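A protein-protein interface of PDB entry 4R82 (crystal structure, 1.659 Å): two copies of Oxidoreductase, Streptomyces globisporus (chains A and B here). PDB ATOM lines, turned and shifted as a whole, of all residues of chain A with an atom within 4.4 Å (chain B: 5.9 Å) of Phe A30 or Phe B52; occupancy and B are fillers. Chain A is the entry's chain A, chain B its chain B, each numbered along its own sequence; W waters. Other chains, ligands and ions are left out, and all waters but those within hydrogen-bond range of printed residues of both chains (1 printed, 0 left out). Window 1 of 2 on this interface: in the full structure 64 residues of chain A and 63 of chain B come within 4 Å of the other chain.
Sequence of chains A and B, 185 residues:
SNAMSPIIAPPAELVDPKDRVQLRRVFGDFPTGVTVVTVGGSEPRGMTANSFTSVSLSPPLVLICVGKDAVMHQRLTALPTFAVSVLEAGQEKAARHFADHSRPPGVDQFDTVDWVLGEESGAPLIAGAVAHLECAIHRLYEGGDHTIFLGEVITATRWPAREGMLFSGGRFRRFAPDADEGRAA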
ATOM      1  N   VAL A  26     -32.068 -21.429  -5.726  1.00  0.00           N
ATOM      2  CA  VAL A  26     -30.999 -20.969  -6.621  1.00  0.00           C
ATOM      3  C   VAL A  26     -30.450 -22.100  -7.496  1.00  0.00           C
ATOM      4  O   VAL A  26     -30.091 -21.866  -8.659  1.00  0.00           O
ATOM      5  CB  VAL A  26     -29.876 -20.179  -5.883  1.00  0.00           C
ATOM      6  CG1 VAL A  26     -29.002 -21.104  -5.071  1.00  0.00           C
ATOM      7  CG2 VAL A  26     -29.032 -19.398  -6.890  1.00  0.00           C
ATOM      8  N   PHE A  27     -30.400 -23.326  -6.969  1.00  0.00           N
ATOM      9  CA  PHE A  27     -30.017 -24.453  -7.814  1.00  0.00           C
ATOM     10  C   PHE A  27     -30.990 -24.584  -8.987  1.00  0.00           C
ATOM     11  O   PHE A  27     -30.586 -24.916 -10.118  1.00  0.00           O
ATOM     12  CB  PHE A  27     -29.988 -25.767  -7.025  1.00  0.00           C
ATOM     13  CG  PHE A  27     -28.778 -25.932  -6.136  1.00  0.00           C
ATOM     14  CD1 PHE A  27     -27.744 -25.009  -6.155  1.00  0.00           C
ATOM     15  CD2 PHE A  27     -28.672 -27.041  -5.302  1.00  0.00           C
ATOM     16  CE1 PHE A  27     -26.630 -25.176  -5.335  1.00  0.00           C
ATOM     17  CE2 PHE A  27     -27.551 -27.226  -4.495  1.00  0.00           C
ATOM     18  CZ  PHE A  27     -26.533 -26.291  -4.516  1.00  0.00           C
ATOM     19  N   GLY A  28     -32.263 -24.293  -8.724  1.00  0.00           N
ATOM     20  CA  GLY A  28     -33.301 -24.412  -9.733  1.00  0.00           C
ATOM     21  C   GLY A  28     -33.214 -23.350 -10.812  1.00  0.00           C
ATOM     22  O   GLY A  28     -33.872 -23.468 -11.862  1.00  0.00           O
ATOM     23  N   ASP A  29     -32.417 -22.310 -10.567  1.00  0.00           N
ATOM     24  CA  ASP A  29     -32.263 -21.237 -11.548  1.00  0.00           C
ATOM     25  C   ASP A  29     -31.448 -21.663 -12.776  1.00  0.00           C
ATOM     26  O   ASP A  29     -31.569 -21.050 -13.831  1.00  0.00           O
ATOM     27  CB  ASP A  29     -31.650 -19.981 -10.923  1.00  0.00           C
ATOM     28  CG  ASP A  29     -32.608 -19.252 -10.022  1.00  0.00           C
ATOM     29  OD1 ASP A  29     -33.831 -19.268 -10.288  1.00  0.00           O
ATOM     30  OD2 ASP A  29     -32.127 -18.636  -9.056  1.00  0.00           O
ATOM     31  N   PHE A  30     -30.624 -22.694 -12.641  1.00  0.00           N
ATOM     32  CA  PHE A  30     -29.909 -23.230 -13.798  1.00  0.00           C
ATOM     33  C   PHE A  30     -30.734 -24.346 -14.419  1.00  0.00           C
ATOM     34  O   PHE A  30     -30.930 -25.398 -13.801  1.00  0.00           O
ATOM     35  CB  PHE A  30     -28.535 -23.758 -13.386  1.00  0.00           C
ATOM     36  CG  PHE A  30     -27.723 -24.289 -14.538  1.00  0.00           C
ATOM     37  CD1 PHE A  30     -27.057 -23.414 -15.388  1.00  0.00           C
ATOM     38  CD2 PHE A  30     -27.622 -25.652 -14.765  1.00  0.00           C
ATOM     39  CE1 PHE A  30     -26.296 -23.890 -16.446  1.00  0.00           C
ATOM     40  CE2 PHE A  30     -26.866 -26.136 -15.826  1.00  0.00           C
ATOM     41  CZ  PHE A  30     -26.211 -25.252 -16.669  1.00  0.00           C
ATOM     42  N   PRO A  31     -31.213 -24.131 -15.657  1.00  0.00           N
ATOM     43  CA  PRO A  31     -32.083 -25.105 -16.327  1.00  0.00           C
ATOM     44  C   PRO A  31     -31.302 -26.330 -16.759  1.00  0.00           C
ATOM     45  O   PRO A  31     -30.119 -26.213 -17.091  1.00  0.00           O
ATOM     46  CB  PRO A  31     -32.543 -24.365 -17.595  1.00  0.00           C
ATOM     47  CG  PRO A  31     -32.123 -22.935 -17.423  1.00  0.00           C
ATOM     48  CD  PRO A  31     -30.975 -22.929 -16.481  1.00  0.00           C
ATOM     49  N   THR A  32     -31.942 -27.496 -16.744  1.00  0.00           N
ATOM     50  CA  THR A  32     -31.303 -28.705 -17.241  1.00  0.00           C
ATOM     51  C   THR A  32     -32.317 -29.569 -17.979  1.00  0.00           C
ATOM     52  O   THR A  32     -33.524 -29.339 -17.904  1.00  0.00           O
ATOM     53  CB  THR A  32     -30.742 -29.571 -16.086  1.00  0.00           C
ATOM     54  OG1 THR A  32     -31.829 -30.098 -15.326  1.00  0.00           O
ATOM     55  CG2 THR A  32     -29.835 -28.769 -15.155  1.00  0.00           C
ATOM     56  N   THR B  32     -29.055 -27.807 -21.403  1.00  0.00           N
ATOM     57  CA  THR B  32     -28.537 -27.144 -20.210  1.00  0.00           C
ATOM     58  C   THR B  32     -28.810 -25.649 -20.283  1.00  0.00           C
ATOM     59  O   THR B  32     -29.169 -25.115 -21.335  1.00  0.00           O
ATOM     60  CB  THR B  32     -26.994 -27.310 -20.082  1.00  0.00           C
ATOM     61  OG1 THR B  32     -26.355 -26.548 -21.111  1.00  0.00           O
ATOM     62  CG2 THR B  32     -26.566 -28.777 -20.198  1.00  0.00           C
ATOM     63  N   GLY B  33     -28.630 -24.965 -19.157  1.00  0.00           N
ATOM     64  CA  GLY B  33     -28.516 -23.521 -19.187  1.00  0.00           C
ATOM     65  C   GLY B  33     -27.103 -23.134 -19.583  1.00  0.00           C
ATOM     66  O   GLY B  33     -26.332 -23.956 -20.081  1.00  0.00           O
ATOM     67  N   VAL B  34     -26.765 -21.869 -19.380  1.00  0.00           N
ATOM     68  CA  VAL B  34     -25.453 -21.353 -19.727  1.00  0.00           C
ATOM     69  C   VAL B  34     -25.032 -20.399 -18.627  1.00  0.00           C
ATOM     70  O   VAL B  34     -25.835 -19.573 -18.171  1.00  0.00           O
ATOM     71  CB  VAL B  34     -25.492 -20.555 -21.048  1.00  0.00           C
ATOM     72  CG1 VAL B  34     -24.085 -20.094 -21.414  1.00  0.00           C
ATOM     73  CG2 VAL B  34     -26.089 -21.389 -22.180  1.00  0.00           C
ATOM     74  N   THR B  35     -23.788 -20.529 -18.185  1.00  0.00           N
ATOM     75  CA  THR B  35     -23.249 -19.630 -17.177  1.00  0.00           C
ATOM     76  C   THR B  35     -22.035 -18.913 -17.721  1.00  0.00           C
ATOM     77  O   THR B  35     -21.465 -19.313 -18.744  1.00  0.00           O
ATOM     78  CB  THR B  35     -22.818 -20.390 -15.904  1.00  0.00           C
ATOM     79  OG1 THR B  35     -21.598 -21.108 -16.159  1.00  0.00           O
ATOM     80  CG2 THR B  35     -23.909 -21.368 -15.458  1.00  0.00           C
ATOM     81  N   ALA B  49     -19.565 -21.380 -19.614  1.00  0.00           N
ATOM     82  CA  ALA B  49     -19.555 -22.772 -19.174  1.00  0.00           C
ATOM     83  C   ALA B  49     -20.981 -23.285 -19.042  1.00  0.00           C
ATOM     84  O   ALA B  49     -21.827 -22.626 -18.415  1.00  0.00           O
ATOM     85  CB  ALA B  49     -18.828 -22.894 -17.837  1.00  0.00           C
ATOM     86  N   ASN B  50     -21.248 -24.453 -19.614  1.00  0.00           N
ATOM     87  CA  ASN B  50     -22.529 -25.121 -19.410  1.00  0.00           C
ATOM     88  C   ASN B  50     -22.385 -26.395 -18.566  1.00  0.00           C
ATOM     89  O   ASN B  50     -23.372 -27.083 -18.287  1.00  0.00           O
ATOM     90  CB  ASN B  50     -23.223 -25.422 -20.754  1.00  0.00           C
ATOM     91  CG  ASN B  50     -22.655 -26.640 -21.454  1.00  0.00           C
ATOM     92  OD1 ASN B  50     -21.442 -26.884 -21.445  1.00  0.00           O
ATOM     93  ND2 ASN B  50     -23.538 -27.418 -22.078  1.00  0.00           N
ATOM     94  N   SER B  51     -21.158 -26.705 -18.139  1.00  0.00           N
ATOM     95  CA  SER B  51     -20.927 -27.902 -17.330  1.00  0.00           C
ATOM     96  C   SER B  51     -21.223 -27.654 -15.853  1.00  0.00           C
ATOM     97  O   SER B  51     -20.973 -28.516 -15.015  1.00  0.00           O
ATOM     98  CB  SER B  51     -19.490 -28.406 -17.486  1.00  0.00           C
ATOM     99  OG  SER B  51     -18.578 -27.384 -17.128  1.00  0.00           O
ATOM    100  N   PHE B  52     -21.764 -26.484 -15.546  1.00  0.00           N
ATOM    101  CA  PHE B  52     -22.182 -26.183 -14.184  1.00  0.00           C
ATOM    102  C   PHE B  52     -23.208 -27.197 -13.721  1.00  0.00           C
ATOM    103  O   PHE B  52     -24.162 -27.497 -14.442  1.00  0.00           O
ATOM    104  CB  PHE B  52     -22.799 -24.790 -14.131  1.00  0.00           C
ATOM    105  CG  PHE B  52     -23.387 -24.455 -12.802  1.00  0.00           C
ATOM    106  CD1 PHE B  52     -22.583 -23.955 -11.783  1.00  0.00           C
ATOM    107  CD2 PHE B  52     -24.732 -24.681 -12.550  1.00  0.00           C
ATOM    108  CE1 PHE B  52     -23.119 -23.653 -10.546  1.00  0.00           C
ATOM    109  CE2 PHE B  52     -25.278 -24.393 -11.307  1.00  0.00           C
ATOM    110  CZ  PHE B  52     -24.476 -23.877 -10.308  1.00  0.00           C
ATOM    111  N   THR B  53     -23.024 -27.702 -12.504  1.00  0.00           N
ATOM    112  CA  THR B  53     -23.907 -28.713 -11.948  1.00  0.00           C
ATOM    113  C   THR B  53     -24.019 -28.458 -10.457  1.00  0.00           C
ATOM    114  O   THR B  53     -23.003 -28.266  -9.795  1.00  0.00           O
ATOM    115  CB  THR B  53     -23.292 -30.091 -12.151  1.00  0.00           C
ATOM    116  OG1 THR B  53     -23.099 -30.315 -13.558  1.00  0.00           O
ATOM    117  CG2 THR B  53     -24.181 -31.180 -11.594  1.00  0.00           C
ATOM    118  N   SER B  54     -25.232 -28.441  -9.923  1.00  0.00           N
ATOM    119  CA  SER B  54     -25.358 -28.351  -8.477  1.00  0.00           C
ATOM    120  C   SER B  54     -25.243 -29.756  -7.894  1.00  0.00           C
ATOM    121  O   SER B  54     -25.811 -30.717  -8.435  1.00  0.00           O
ATOM    122  CB  SER B  54     -26.650 -27.648  -8.079  1.00  0.00           C
ATOM    123  OG  SER B  54     -27.776 -28.171  -8.764  1.00  0.00           O
ATOM    124  N   VAL B  62     -21.275 -26.973  -5.665  1.00  0.00           N
ATOM    125  CA  VAL B  62     -21.529 -27.004  -7.107  1.00  0.00           C
ATOM    126  C   VAL B  62     -20.231 -27.434  -7.768  1.00  0.00           C
ATOM    127  O   VAL B  62     -19.174 -27.423  -7.128  1.00  0.00           O
ATOM    128  CB  VAL B  62     -21.948 -25.618  -7.651  1.00  0.00           C
ATOM    129  CG1 VAL B  62     -23.251 -25.144  -7.018  1.00  0.00           C
ATOM    130  CG2 VAL B  62     -20.819 -24.588  -7.437  1.00  0.00           C
ATOM    131  N   LEU B  63     -20.295 -27.827  -9.035  1.00  0.00           N
ATOM    132  CA  LEU B  63     -19.063 -28.099  -9.774  1.00  0.00           C
ATOM    133  C   LEU B  63     -19.111 -27.485 -11.160  1.00  0.00           C
ATOM    134  O   LEU B  63     -20.192 -27.179 -11.684  1.00  0.00           O
ATOM    135  CB  LEU B  63     -18.752 -29.609  -9.870  1.00  0.00           C
ATOM    136  CG  LEU B  63     -19.694 -30.579 -10.599  1.00  0.00           C
ATOM    137  CD1 LEU B  63     -19.552 -30.467 -12.126  1.00  0.00           C
ATOM    138  CD2 LEU B  63     -19.424 -32.019 -10.171  1.00  0.00           C
ATOM    139  N   ILE B  64     -17.927 -27.314 -11.746  1.00  0.00           N
ATOM    140  CA  ILE B  64     -17.810 -26.945 -13.149  1.00  0.00           C
ATOM    141  C   ILE B  64     -16.683 -27.780 -13.715  1.00  0.00           C
ATOM    142  O   ILE B  64     -15.776 -28.192 -12.971  1.00  0.00           O
ATOM    143  CB  ILE B  64     -17.525 -25.441 -13.358  1.00  0.00           C
ATOM    144  CG1 ILE B  64     -16.303 -25.002 -12.552  1.00  0.00           C
ATOM    145  CG2 ILE B  64     -18.751 -24.592 -12.988  1.00  0.00           C
ATOM    146  CD1 ILE B  64     -15.900 -23.540 -12.788  1.00  0.00           C
ATOM    147  N   CYS B  65     -16.764 -28.070 -15.010  1.00  0.00           N
ATOM    148  CA  CYS B  65     -15.726 -28.826 -15.690  1.00  0.00           C
ATOM    149  C   CYS B  65     -15.024 -27.890 -16.657  1.00  0.00           C
ATOM    150  O   CYS B  65     -15.670 -27.286 -17.515  1.00  0.00           O
ATOM    151  CB  CYS B  65     -16.333 -29.990 -16.464  1.00  0.00           C
ATOM    152  SG  CYS B  65     -17.268 -31.124 -15.399  1.00  0.00           S
ATOM    153  N   VAL B  84     -20.168 -17.588 -10.415  1.00  0.00           N
ATOM    154  CA  VAL B  84     -20.931 -18.158 -11.513  1.00  0.00           C
ATOM    155  C   VAL B  84     -22.111 -17.235 -11.751  1.00  0.00           C
ATOM    156  O   VAL B  84     -22.857 -16.946 -10.816  1.00  0.00           O
ATOM    157  CB  VAL B  84     -21.479 -19.542 -11.144  1.00  0.00           C
ATOM    158  CG1 VAL B  84     -22.362 -20.094 -12.283  1.00  0.00           C
ATOM    159  CG2 VAL B  84     -20.345 -20.492 -10.825  1.00  0.00           C
ATOM    160  N   VAL B  86     -25.497 -17.161 -13.822  1.00  0.00           N
ATOM    161  CA  VAL B  86     -26.393 -17.959 -14.648  1.00  0.00           C
ATOM    162  C   VAL B  86     -27.076 -17.019 -15.623  1.00  0.00           C
ATOM    163  O   VAL B  86     -27.779 -16.107 -15.205  1.00  0.00           O
ATOM    164  CB  VAL B  86     -27.459 -18.668 -13.802  1.00  0.00           C
ATOM    165  CG1 VAL B  86     -28.437 -19.414 -14.711  1.00  0.00           C
ATOM    166  CG2 VAL B  86     -26.795 -19.638 -12.829  1.00  0.00           C
ATOM    167  N   LEU B 133     -23.666 -16.876  -8.089  1.00  0.00           N
ATOM    168  CA  LEU B 133     -23.215 -17.714  -6.987  1.00  0.00           C
ATOM    169  C   LEU B 133     -21.731 -17.439  -6.792  1.00  0.00           C
ATOM    170  O   LEU B 133     -20.952 -17.527  -7.735  1.00  0.00           O
ATOM    171  CB  LEU B 133     -23.426 -19.199  -7.290  1.00  0.00           C
ATOM    172  CG  LEU B 133     -24.861 -19.682  -7.490  1.00  0.00           C
ATOM    173  CD1 LEU B 133     -25.316 -19.479  -8.945  1.00  0.00           C
ATOM    174  CD2 LEU B 133     -24.995 -21.145  -7.095  1.00  0.00           C
HETATM  175  O   HOH W   1     -28.786 -26.920 -10.994  1.00  0.00           O
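The backbone NH of Gly B33 is in hydrogen-bond range of the backbone carbonyl oxygen of Pro A31, 2.8 Å away.
Printed residues of chain B within 4 Å of Phe A27: Ser B54 (3.4 Å) and Val B62 (3.8 Å). Phe A30 touches just these residues of chain B: Gly B33, Val B34, Thr B35, Asn B50 and Phe B52. Printed residues of chain A within 4 Å of Thr B32: Pro A31 (3.5 Å). Phe B52 touches one residue of chain A. The nearest printed residue of chain A that does not touch Phe B52 is Phe A27 (5.4 Å). The nearest printed residue of chain B that does not touch Pro A31 is Val B86 (4.7 Å).
Of the 7 printed residues of chain A, 4 touch a printed residue of chain B. Hydrophobic or aromatic side chains of chain A that line the printed part of chain B: Phe A27, Phe A30 and Pro A31. Hydrophobic or aromatic side chains of chain B within 4 Å of the printed part of chain A: Phe B52, Val B62 and Val B86. Along chain B the printed residues that touch a printed residue of chain A span positions 32 to 86. Among the printed residues, no Asp or Glu carboxylate lies within 4 Å of a Lys or Arg side-chain nitrogen of the other chain.
Ser B54 touches Phe A27. Val B62 touches Phe A27 (CG1 to CE1, 3.8 Å). Asp A29 touches Val B86 (O to CG1, 3.6 Å). Gly B33 touches Phe A30. Val B34 touches Phe A30 (N to CE1, 3.6 Å). Phe A30 touches Thr B35 (CE1 to CG2, 3.6 Å). CZ of Phe A30 touches O of Asn B50, at 3.7 Å. Phe A30 touches Phe B52. Thr B32 touches Pro A31.
Water W1 bridges OG of Ser B54 and O of Phe A27.
Position printed for both chains: 32. Of the 10 pairs that touch across the chains among the printed residues, none has its exchanged pair printed and touching as well.
ND2 of Asn B50 is in hydrogen-bond range of OG1 of Thr B32 (3.1 Å). The side-chain hydroxyl (OG1) of Thr B35 sits at hydrogen-bond distance from the backbone carbonyl oxygen (O) of Ala B49, at 2.7 Å.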
